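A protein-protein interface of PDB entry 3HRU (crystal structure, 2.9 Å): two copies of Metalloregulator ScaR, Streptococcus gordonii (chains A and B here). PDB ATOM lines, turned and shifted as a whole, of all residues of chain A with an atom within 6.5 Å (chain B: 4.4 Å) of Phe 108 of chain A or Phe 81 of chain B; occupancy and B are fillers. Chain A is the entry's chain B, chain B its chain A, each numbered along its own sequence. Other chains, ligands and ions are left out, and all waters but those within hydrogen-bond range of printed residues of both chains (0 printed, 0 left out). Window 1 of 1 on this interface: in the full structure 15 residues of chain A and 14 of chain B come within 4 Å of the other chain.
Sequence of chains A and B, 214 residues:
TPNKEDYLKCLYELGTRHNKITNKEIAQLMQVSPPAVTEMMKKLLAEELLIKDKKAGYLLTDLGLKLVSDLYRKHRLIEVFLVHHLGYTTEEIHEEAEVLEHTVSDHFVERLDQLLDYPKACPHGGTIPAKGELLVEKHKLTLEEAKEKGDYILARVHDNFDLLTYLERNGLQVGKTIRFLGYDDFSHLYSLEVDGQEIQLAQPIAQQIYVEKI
The side-chain carboxylate (OE1) of Glu 96 of chain B is in hydrogen-bond range of the side-chain hydroxyl (OG) of Ser 105 of chain A (2.5 Å).
Among the printed residues, pairs that only touch across the chains: His 107 of chain A with Glu 96 of chain B (3.0 Å), Phe 108 of chain A with Tyr 88 of chain B (3.4 Å), His 107 of chain A with Tyr 88 of chain B (3.4 Å), Arg 111 of chain A with Leu 86 of chain B (3.5 Å), Leu 115 of chain A with His 85 of chain B (3.7 Å), Phe 81 of chain A with Phe 81 of chain B (3.7 Å), Phe 108 of chain A with Leu 86 of chain B (3.9 Å), Phe 108 of chain A with Phe 81 of chain B (3.9 Å), Phe 108 of chain A with Leu 100 of chain B (3.9 Å), Leu 112 of chain A with Leu 86 of chain B (3.96 Å) and Phe 108 of chain A with Leu 82 of chain B (3.996 Å).
N of His 107 of chain A lies close to OG of Ser 105 of chain A (3.3 Å).
The backbone carbonyl oxygen (O) of Phe 81 of chain B lies within hydrogen-bond range of the backbone NH (N) of Leu 86 of chain B.
N of Tyr 88 of chain B is in hydrogen-bond range of O of Leu 82 of chain B (3.0 Å).
The backbone NH (N) of Phe 108 of chain A lies within hydrogen-bond range of the side-chain hydroxyl (OG) of Ser 105 of chain A, at 3.1 Å.
The side-chain hydroxyl (OH) of Tyr 88 of chain B is in hydrogen-bond range of the side-chain carboxylate (OE1) of Glu 96 of chain B (2.8 Å).
Of the 15 printed residues of chain B, 7 touch a printed residue of chain A.
Of the 14 printed residues of chain A, 7 touch a printed residue of chain B.
Hydrophobic or aromatic side chains of chain A that line the printed part of chain B: Phe 81, His 107, Phe 108 and Leu 115.
Among the printed residues, 12 pairs touch across the chains.
Glu 110 of chain A touches none of the printed residues of chain B.
Printed residues of chain B within 4 Å of Arg 111 of chain A: Leu 86 (3.5 Å).
Printed residues of chain A within 4 Å of Leu 86 of chain B: Phe 108, Arg 111 and Leu 112.
Printed residues of chain A within 4 Å of Glu 96 of chain B: Ser 105 and His 107.
Printed residues of chain A within 4 Å of Leu 100 of chain B: Phe 108.
Leu 116 of chain B touches none of the printed residues of chain A.
The nearest residue of chain A that does not touch Phe 81 of chain B is Leu 115 of chain A (4.6 Å).
The nearest printed residue of chain B that does not touch Leu 112 of chain A is Phe 81 of chain B (5.4 Å).
Phe 81 of chain A touches its own counterpart, Phe 81 of chain B.
4 positions are printed for both chains.
Of the 12 pairs that touch across the chains among the printed residues, 1 has its exchanged pair printed and touching as well.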
ATOM      1  N   ILE A  78      12.553  17.317  -4.203  1.00  0.00           N
ATOM      2  CA  ILE A  78      11.362  16.550  -4.490  1.00  0.00           C
ATOM      3  C   ILE A  78      11.459  15.957  -5.887  1.00  0.00           C
ATOM      4  O   ILE A  78      11.053  14.824  -6.141  1.00  0.00           O
ATOM      5  CB  ILE A  78      10.116  17.426  -4.454  1.00  0.00           C
ATOM      6  CG1 ILE A  78       9.862  17.890  -3.034  1.00  0.00           C
ATOM      7  CG2 ILE A  78       8.918  16.665  -5.000  1.00  0.00           C
ATOM      8  CD1 ILE A  78       9.725  16.751  -2.061  1.00  0.00           C
ATOM      9  N   PHE A  81      13.851  13.053  -5.951  1.00  0.00           N
ATOM     10  CA  PHE A  81      13.325  11.909  -5.226  1.00  0.00           C
ATOM     11  C   PHE A  81      12.307  11.229  -6.094  1.00  0.00           C
ATOM     12  O   PHE A  81      12.405  10.030  -6.347  1.00  0.00           O
ATOM     13  CB  PHE A  81      12.688  12.315  -3.891  1.00  0.00           C
ATOM     14  CG  PHE A  81      11.974  11.181  -3.187  1.00  0.00           C
ATOM     15  CD1 PHE A  81      12.679  10.106  -2.676  1.00  0.00           C
ATOM     16  CD2 PHE A  81      10.604  11.180  -3.055  1.00  0.00           C
ATOM     17  CE1 PHE A  81      12.039   9.053  -2.048  1.00  0.00           C
ATOM     18  CE2 PHE A  81       9.950  10.103  -2.416  1.00  0.00           C
ATOM     19  CZ  PHE A  81      10.677   9.054  -1.914  1.00  0.00           C
ATOM     20  N   LEU A 100       2.739  18.261  -3.094  1.00  0.00           N
ATOM     21  CA  LEU A 100       3.424  17.798  -1.896  1.00  0.00           C
ATOM     22  C   LEU A 100       4.643  18.641  -1.668  1.00  0.00           C
ATOM     23  O   LEU A 100       5.119  18.768  -0.547  1.00  0.00           O
ATOM     24  CB  LEU A 100       3.750  16.306  -1.943  1.00  0.00           C
ATOM     25  CG  LEU A 100       4.954  15.695  -2.642  1.00  0.00           C
ATOM     26  CD1 LEU A 100       5.232  14.425  -1.891  1.00  0.00           C
ATOM     27  CD2 LEU A 100       4.660  15.394  -4.081  1.00  0.00           C
ATOM     28  N   VAL A 104       5.164  19.178   2.226  1.00  0.00           N
ATOM     29  CA  VAL A 104       6.329  18.700   2.975  1.00  0.00           C
ATOM     30  C   VAL A 104       7.073  19.784   3.724  1.00  0.00           C
ATOM     31  O   VAL A 104       7.481  20.783   3.139  1.00  0.00           O
ATOM     32  CB  VAL A 104       7.359  17.968   2.078  1.00  0.00           C
ATOM     33  CG1 VAL A 104       6.760  16.690   1.517  1.00  0.00           C
ATOM     34  CG2 VAL A 104       7.854  18.874   0.978  1.00  0.00           C
ATOM     35  N   SER A 105       7.260  19.557   5.020  1.00  0.00           N
ATOM     36  CA  SER A 105       8.020  20.457   5.890  1.00  0.00           C
ATOM     37  C   SER A 105       9.500  20.642   5.486  1.00  0.00           C
ATOM     38  O   SER A 105      10.035  19.887   4.675  1.00  0.00           O
ATOM     39  CB  SER A 105       7.985  19.914   7.311  1.00  0.00           C
ATOM     40  OG  SER A 105       8.751  18.732   7.365  1.00  0.00           O
ATOM     41  N   ASP A 106      10.169  21.637   6.069  1.00  0.00           N
ATOM     42  CA  ASP A 106      11.602  21.774   5.852  1.00  0.00           C
ATOM     43  C   ASP A 106      12.334  20.555   6.407  1.00  0.00           C
ATOM     44  O   ASP A 106      13.359  20.142   5.878  1.00  0.00           O
ATOM     45  CB  ASP A 106      12.153  23.053   6.490  1.00  0.00           C
ATOM     46  CG  ASP A 106      11.810  24.318   5.690  1.00  0.00           C
ATOM     47  OD1 ASP A 106      11.655  25.376   6.343  1.00  0.00           O
ATOM     48  OD2 ASP A 106      11.704  24.263   4.428  1.00  0.00           O
ATOM     49  N   HIS A 107      11.807  19.973   7.480  1.00  0.00           N
ATOM     50  CA  HIS A 107      12.437  18.792   8.069  1.00  0.00           C
ATOM     51  C   HIS A 107      12.508  17.640   7.049  1.00  0.00           C
ATOM     52  O   HIS A 107      13.561  17.023   6.847  1.00  0.00           O
ATOM     53  CB  HIS A 107      11.718  18.383   9.355  1.00  0.00           C
ATOM     54  CG  HIS A 107      12.170  17.065   9.903  1.00  0.00           C
ATOM     55  ND1 HIS A 107      13.502  16.750  10.076  1.00  0.00           N
ATOM     56  CD2 HIS A 107      11.468  15.976  10.314  1.00  0.00           C
ATOM     57  CE1 HIS A 107      13.599  15.527  10.574  1.00  0.00           C
ATOM     58  NE2 HIS A 107      12.381  15.034  10.722  1.00  0.00           N
ATOM     59  N   PHE A 108      11.375  17.377   6.402  1.00  0.00           N
ATOM     60  CA  PHE A 108      11.275  16.379   5.350  1.00  0.00           C
ATOM     61  C   PHE A 108      12.357  16.661   4.298  1.00  0.00           C
ATOM     62  O   PHE A 108      13.154  15.783   3.945  1.00  0.00           O
ATOM     63  CB  PHE A 108       9.874  16.439   4.739  1.00  0.00           C
ATOM     64  CG  PHE A 108       9.597  15.372   3.725  1.00  0.00           C
ATOM     65  CD1 PHE A 108       8.985  14.177   4.099  1.00  0.00           C
ATOM     66  CD2 PHE A 108       9.912  15.570   2.389  1.00  0.00           C
ATOM     67  CE1 PHE A 108       8.718  13.186   3.159  1.00  0.00           C
ATOM     68  CE2 PHE A 108       9.644  14.589   1.440  1.00  0.00           C
ATOM     69  CZ  PHE A 108       9.051  13.396   1.832  1.00  0.00           C
ATOM     70  N   VAL A 109      12.407  17.899   3.812  1.00  0.00           N
ATOM     71  CA  VAL A 109      13.338  18.238   2.763  1.00  0.00           C
ATOM     72  C   VAL A 109      14.770  18.063   3.283  1.00  0.00           C
ATOM     73  O   VAL A 109      15.639  17.581   2.567  1.00  0.00           O
ATOM     74  CB  VAL A 109      13.048  19.638   2.228  1.00  0.00           C
ATOM     75  CG1 VAL A 109      13.981  19.997   1.071  1.00  0.00           C
ATOM     76  CG2 VAL A 109      11.616  19.691   1.771  1.00  0.00           C
ATOM     77  N   GLU A 110      15.016  18.413   4.538  1.00  0.00           N
ATOM     78  CA  GLU A 110      16.354  18.240   5.080  1.00  0.00           C
ATOM     79  C   GLU A 110      16.783  16.778   5.086  1.00  0.00           C
ATOM     80  O   GLU A 110      17.940  16.478   4.807  1.00  0.00           O
ATOM     81  CB  GLU A 110      16.482  18.838   6.481  1.00  0.00           C
ATOM     82  CG  GLU A 110      17.349  20.077   6.539  1.00  0.00           C
ATOM     83  CD  GLU A 110      16.852  21.187   5.612  1.00  0.00           C
ATOM     84  OE1 GLU A 110      16.102  22.069   6.108  1.00  0.00           O
ATOM     85  OE2 GLU A 110      17.201  21.178   4.396  1.00  0.00           O
ATOM     86  N   ARG A 111      15.860  15.866   5.397  1.00  0.00           N
ATOM     87  CA  ARG A 111      16.231  14.462   5.534  1.00  0.00           C
ATOM     88  C   ARG A 111      16.282  13.785   4.179  1.00  0.00           C
ATOM     89  O   ARG A 111      17.107  12.917   3.942  1.00  0.00           O
ATOM     90  CB  ARG A 111      15.298  13.736   6.491  1.00  0.00           C
ATOM     91  CG  ARG A 111      15.265  14.326   7.897  1.00  0.00           C
ATOM     92  CD  ARG A 111      16.675  14.469   8.496  1.00  0.00           C
ATOM     93  NE  ARG A 111      17.101  13.346   9.340  1.00  0.00           N
ATOM     94  CZ  ARG A 111      17.718  12.245   8.898  1.00  0.00           C
ATOM     95  NH1 ARG A 111      17.986  12.055   7.594  1.00  0.00           N
ATOM     96  NH2 ARG A 111      18.056  11.309   9.778  1.00  0.00           N
ATOM     97  N   LEU A 112      15.400  14.204   3.283  1.00  0.00           N
ATOM     98  CA  LEU A 112      15.445  13.792   1.895  1.00  0.00           C
ATOM     99  C   LEU A 112      16.800  14.146   1.312  1.00  0.00           C
ATOM    100  O   LEU A 112      17.365  13.401   0.521  1.00  0.00           O
ATOM    101  CB  LEU A 112      14.407  14.577   1.137  1.00  0.00           C
ATOM    102  CG  LEU A 112      13.530  13.784   0.190  1.00  0.00           C
ATOM    103  CD1 LEU A 112      13.083  14.714  -0.928  1.00  0.00           C
ATOM    104  CD2 LEU A 112      14.288  12.578  -0.349  1.00  0.00           C
ATOM    105  N   ASP A 113      17.317  15.312   1.685  1.00  0.00           N
ATOM    106  CA  ASP A 113      18.582  15.764   1.134  1.00  0.00           C
ATOM    107  C   ASP A 113      19.622  14.770   1.554  1.00  0.00           C
ATOM    108  O   ASP A 113      20.543  14.468   0.823  1.00  0.00           O
ATOM    109  CB  ASP A 113      18.956  17.156   1.641  1.00  0.00           C
ATOM    110  CG  ASP A 113      19.982  17.865   0.739  1.00  0.00           C
ATOM    111  OD1 ASP A 113      20.171  17.450  -0.424  1.00  0.00           O
ATOM    112  OD2 ASP A 113      20.594  18.862   1.182  1.00  0.00           O
ATOM    113  N   LEU A 115      19.111  11.563   2.527  1.00  0.00           N
ATOM    114  CA  LEU A 115      18.892  10.234   1.983  1.00  0.00           C
ATOM    115  C   LEU A 115      19.533  10.183   0.604  1.00  0.00           C
ATOM    116  O   LEU A 115      20.319   9.286   0.307  1.00  0.00           O
ATOM    117  CB  LEU A 115      17.400   9.911   1.893  1.00  0.00           C
ATOM    118  CG  LEU A 115      17.102   8.554   1.278  1.00  0.00           C
ATOM    119  CD1 LEU A 115      17.468   7.418   2.226  1.00  0.00           C
ATOM    120  CD2 LEU A 115      15.639   8.471   0.920  1.00  0.00           C
ATOM    121  N   LEU B  77       2.698   2.496   5.101  1.00  0.00           N
ATOM    122  CA  LEU B  77       3.793   2.693   4.166  1.00  0.00           C
ATOM    123  C   LEU B  77       4.458   4.043   4.421  1.00  0.00           C
ATOM    124  O   LEU B  77       5.692   4.119   4.532  1.00  0.00           O
ATOM    125  CB  LEU B  77       3.295   2.601   2.739  1.00  0.00           C
ATOM    126  CG  LEU B  77       3.026   1.207   2.169  1.00  0.00           C
ATOM    127  CD1 LEU B  77       2.746   1.312   0.677  1.00  0.00           C
ATOM    128  CD2 LEU B  77       4.216   0.334   2.383  1.00  0.00           C
ATOM    129  N   ILE B  78       3.664   5.107   4.543  1.00  0.00           N
ATOM    130  CA  ILE B  78       4.257   6.404   4.824  1.00  0.00           C
ATOM    131  C   ILE B  78       5.076   6.294   6.091  1.00  0.00           C
ATOM    132  O   ILE B  78       6.210   6.784   6.171  1.00  0.00           O
ATOM    133  CB  ILE B  78       3.242   7.501   5.075  1.00  0.00           C
ATOM    134  CG1 ILE B  78       2.464   7.823   3.808  1.00  0.00           C
ATOM    135  CG2 ILE B  78       3.986   8.750   5.501  1.00  0.00           C
ATOM    136  CD1 ILE B  78       3.376   8.182   2.675  1.00  0.00           C
ATOM    137  N   GLU B  79       4.485   5.662   7.095  1.00  0.00           N
ATOM    138  CA  GLU B  79       5.140   5.538   8.372  1.00  0.00           C
ATOM    139  C   GLU B  79       6.492   4.913   8.107  1.00  0.00           C
ATOM    140  O   GLU B  79       7.511   5.497   8.446  1.00  0.00           O
ATOM    141  CB  GLU B  79       4.294   4.676   9.305  1.00  0.00           C
ATOM    142  CG  GLU B  79       4.337   5.113  10.749  1.00  0.00           C
ATOM    143  CD  GLU B  79       2.994   4.905  11.456  1.00  0.00           C
ATOM    144  OE1 GLU B  79       2.721   3.732  11.777  1.00  0.00           O
ATOM    145  OE2 GLU B  79       2.223   5.886  11.704  1.00  0.00           O
ATOM    146  N   VAL B  80       6.503   3.743   7.467  1.00  0.00           N
ATOM    147  CA  VAL B  80       7.745   3.002   7.256  1.00  0.00           C
ATOM    148  C   VAL B  80       8.741   3.844   6.508  1.00  0.00           C
ATOM    149  O   VAL B  80       9.918   3.843   6.815  1.00  0.00           O
ATOM    150  CB  VAL B  80       7.576   1.796   6.354  1.00  0.00           C
ATOM    151  CG1 VAL B  80       8.985   1.221   5.981  1.00  0.00           C
ATOM    152  CG2 VAL B  80       6.644   0.767   6.995  1.00  0.00           C
ATOM    153  N   PHE B  81       8.279   4.543   5.488  1.00  0.00           N
ATOM    154  CA  PHE B  81       9.202   5.373   4.763  1.00  0.00           C
ATOM    155  C   PHE B  81       9.771   6.421   5.709  1.00  0.00           C
ATOM    156  O   PHE B  81      10.976   6.515   5.860  1.00  0.00           O
ATOM    157  CB  PHE B  81       8.526   5.989   3.545  1.00  0.00           C
ATOM    158  CG  PHE B  81       9.292   7.101   2.927  1.00  0.00           C
ATOM    159  CD1 PHE B  81      10.399   6.840   2.148  1.00  0.00           C
ATOM    160  CD2 PHE B  81       8.915   8.419   3.139  1.00  0.00           C
ATOM    161  CE1 PHE B  81      11.127   7.875   1.582  1.00  0.00           C
ATOM    162  CE2 PHE B  81       9.628   9.464   2.579  1.00  0.00           C
ATOM    163  CZ  PHE B  81      10.738   9.194   1.800  1.00  0.00           C
ATOM    164  N   LEU B  82       8.924   7.191   6.373  1.00  0.00           N
ATOM    165  CA  LEU B  82       9.441   8.241   7.262  1.00  0.00           C
ATOM    166  C   LEU B  82      10.505   7.811   8.282  1.00  0.00           C
ATOM    167  O   LEU B  82      11.544   8.477   8.414  1.00  0.00           O
ATOM    168  CB  LEU B  82       8.330   8.964   7.998  1.00  0.00           C
ATOM    169  CG  LEU B  82       7.352   9.667   7.083  1.00  0.00           C
ATOM    170  CD1 LEU B  82       6.357  10.382   7.962  1.00  0.00           C
ATOM    171  CD2 LEU B  82       8.089  10.624   6.160  1.00  0.00           C
ATOM    172  N   VAL B  83      10.261   6.737   9.031  1.00  0.00           N
ATOM    173  CA  VAL B  83      11.246   6.356  10.045  1.00  0.00           C
ATOM    174  C   VAL B  83      12.429   5.570   9.472  1.00  0.00           C
ATOM    175  O   VAL B  83      13.587   5.844   9.796  1.00  0.00           O
ATOM    176  CB  VAL B  83      10.634   5.633  11.310  1.00  0.00           C
ATOM    177  CG1 VAL B  83       9.143   5.530  11.228  1.00  0.00           C
ATOM    178  CG2 VAL B  83      11.263   4.259  11.506  1.00  0.00           C
ATOM    179  N   HIS B  84      12.160   4.593   8.629  1.00  0.00           N
ATOM    180  CA  HIS B  84      13.253   3.800   8.093  1.00  0.00           C
ATOM    181  C   HIS B  84      14.165   4.510   7.107  1.00  0.00           C
ATOM    182  O   HIS B  84      15.362   4.227   7.025  1.00  0.00           O
ATOM    183  CB  HIS B  84      12.687   2.572   7.443  1.00  0.00           C
ATOM    184  CG  HIS B  84      12.409   1.491   8.414  1.00  0.00           C
ATOM    185  ND1 HIS B  84      12.290   0.167   8.048  1.00  0.00           N
ATOM    186  CD2 HIS B  84      12.269   1.529   9.755  1.00  0.00           C
ATOM    187  CE1 HIS B  84      12.086  -0.561   9.126  1.00  0.00           C
ATOM    188  NE2 HIS B  84      12.069   0.242  10.178  1.00  0.00           N
ATOM    189  N   HIS B  85      13.601   5.414   6.333  1.00  0.00           N
ATOM    190  CA  HIS B  85      14.387   6.059   5.319  1.00  0.00           C
ATOM    191  C   HIS B  85      14.825   7.436   5.816  1.00  0.00           C
ATOM    192  O   HIS B  85      15.928   7.860   5.518  1.00  0.00           O
ATOM    193  CB  HIS B  85      13.594   6.149   4.015  1.00  0.00           C
ATOM    194  CG  HIS B  85      13.673   4.914   3.172  1.00  0.00           C
ATOM    195  ND1 HIS B  85      13.931   4.952   1.814  1.00  0.00           N
ATOM    196  CD2 HIS B  85      13.535   3.608   3.488  1.00  0.00           C
ATOM    197  CE1 HIS B  85      13.961   3.720   1.336  1.00  0.00           C
ATOM    198  NE2 HIS B  85      13.712   2.885   2.330  1.00  0.00           N
ATOM    199  N   LEU B  86      13.984   8.132   6.586  1.00  0.00           N
ATOM    200  CA  LEU B  86      14.284   9.528   6.904  1.00  0.00           C
ATOM    201  C   LEU B  86      14.544   9.745   8.402  1.00  0.00           C
ATOM    202  O   LEU B  86      14.482  10.888   8.887  1.00  0.00           O
ATOM    203  CB  LEU B  86      13.160  10.468   6.446  1.00  0.00           C
ATOM    204  CG  LEU B  86      12.746  10.641   4.976  1.00  0.00           C
ATOM    205  CD1 LEU B  86      12.032  11.935   4.874  1.00  0.00           C
ATOM    206  CD2 LEU B  86      13.917  10.608   4.024  1.00  0.00           C
ATOM    207  N   TYR B  88      12.763   9.460  11.020  1.00  0.00           N
ATOM    208  CA  TYR B  88      11.780  10.220  11.810  1.00  0.00           C
ATOM    209  C   TYR B  88      11.629   9.755  13.266  1.00  0.00           C
ATOM    210  O   TYR B  88      11.863   8.590  13.571  1.00  0.00           O
ATOM    211  CB  TYR B  88      10.424  10.221  11.123  1.00  0.00           C
ATOM    212  CG  TYR B  88      10.221  11.404  10.200  1.00  0.00           C
ATOM    213  CD1 TYR B  88      11.123  11.687   9.163  1.00  0.00           C
ATOM    214  CD2 TYR B  88       9.128  12.240  10.365  1.00  0.00           C
ATOM    215  CE1 TYR B  88      10.926  12.777   8.328  1.00  0.00           C
ATOM    216  CE2 TYR B  88       8.929  13.324   9.539  1.00  0.00           C
ATOM    217  CZ  TYR B  88       9.815  13.589   8.530  1.00  0.00           C
ATOM    218  OH  TYR B  88       9.552  14.674   7.736  1.00  0.00           O
ATOM    219  N   GLU B  96       3.797  15.191  11.432  1.00  0.00           N
ATOM    220  CA  GLU B  96       3.880  15.239   9.962  1.00  0.00           C
ATOM    221  C   GLU B  96       3.247  14.109   9.182  1.00  0.00           C
ATOM    222  O   GLU B  96       2.745  14.335   8.091  1.00  0.00           O
ATOM    223  CB  GLU B  96       5.323  15.333   9.496  1.00  0.00           C
ATOM    224  CG  GLU B  96       6.100  16.525  10.013  1.00  0.00           C
ATOM    225  CD  GLU B  96       7.505  16.549   9.453  1.00  0.00           C
ATOM    226  OE1 GLU B  96       7.633  16.682   8.212  1.00  0.00           O
ATOM    227  OE2 GLU B  96       8.471  16.412  10.246  1.00  0.00           O
ATOM    228  N   LEU B 100       0.646  14.182   5.195  1.00  0.00           N
ATOM    229  CA  LEU B 100       1.086  13.577   3.945  1.00  0.00           C
ATOM    230  C   LEU B 100       0.086  12.529   3.455  1.00  0.00           C
ATOM    231  O   LEU B 100      -0.131  12.406   2.248  1.00  0.00           O
ATOM    232  CB  LEU B 100       2.460  12.954   4.078  1.00  0.00           C
ATOM    233  CG  LEU B 100       3.621  13.882   3.817  1.00  0.00           C
ATOM    234  CD1 LEU B 100       3.685  14.937   4.916  1.00  0.00           C
ATOM    235  CD2 LEU B 100       4.895  13.043   3.791  1.00  0.00           C
ATOM    236  N   LEU B 112       6.020   4.115  -3.586  1.00  0.00           N
ATOM    237  CA  LEU B 112       6.669   4.095  -2.293  1.00  0.00           C
ATOM    238  C   LEU B 112       6.772   2.662  -1.865  1.00  0.00           C
ATOM    239  O   LEU B 112       7.774   2.246  -1.283  1.00  0.00           O
ATOM    240  CB  LEU B 112       5.806   4.824  -1.275  1.00  0.00           C
ATOM    241  CG  LEU B 112       6.484   5.717  -0.240  1.00  0.00           C
ATOM    242  CD1 LEU B 112       5.652   5.702   1.021  1.00  0.00           C
ATOM    243  CD2 LEU B 112       7.866   5.246   0.034  1.00  0.00           C
ATOM    244  N   LEU B 116      10.179   0.709  -0.973  1.00  0.00           N
ATOM    245  CA  LEU B 116      10.368   0.139   0.348  1.00  0.00           C
ATOM    246  C   LEU B 116      10.517  -1.395   0.292  1.00  0.00           C
ATOM    247  O   LEU B 116      10.646  -2.076   1.309  1.00  0.00           O
ATOM    248  CB  LEU B 116       9.228   0.565   1.255  1.00  0.00           C
ATOM    249  CG  LEU B 116       9.067   2.057   1.541  1.00  0.00           C
ATOM    250  CD1 LEU B 116       8.024   2.215   2.657  1.00  0.00           C
ATOM    251  CD2 LEU B 116      10.374   2.704   1.951  1.00  0.00           C
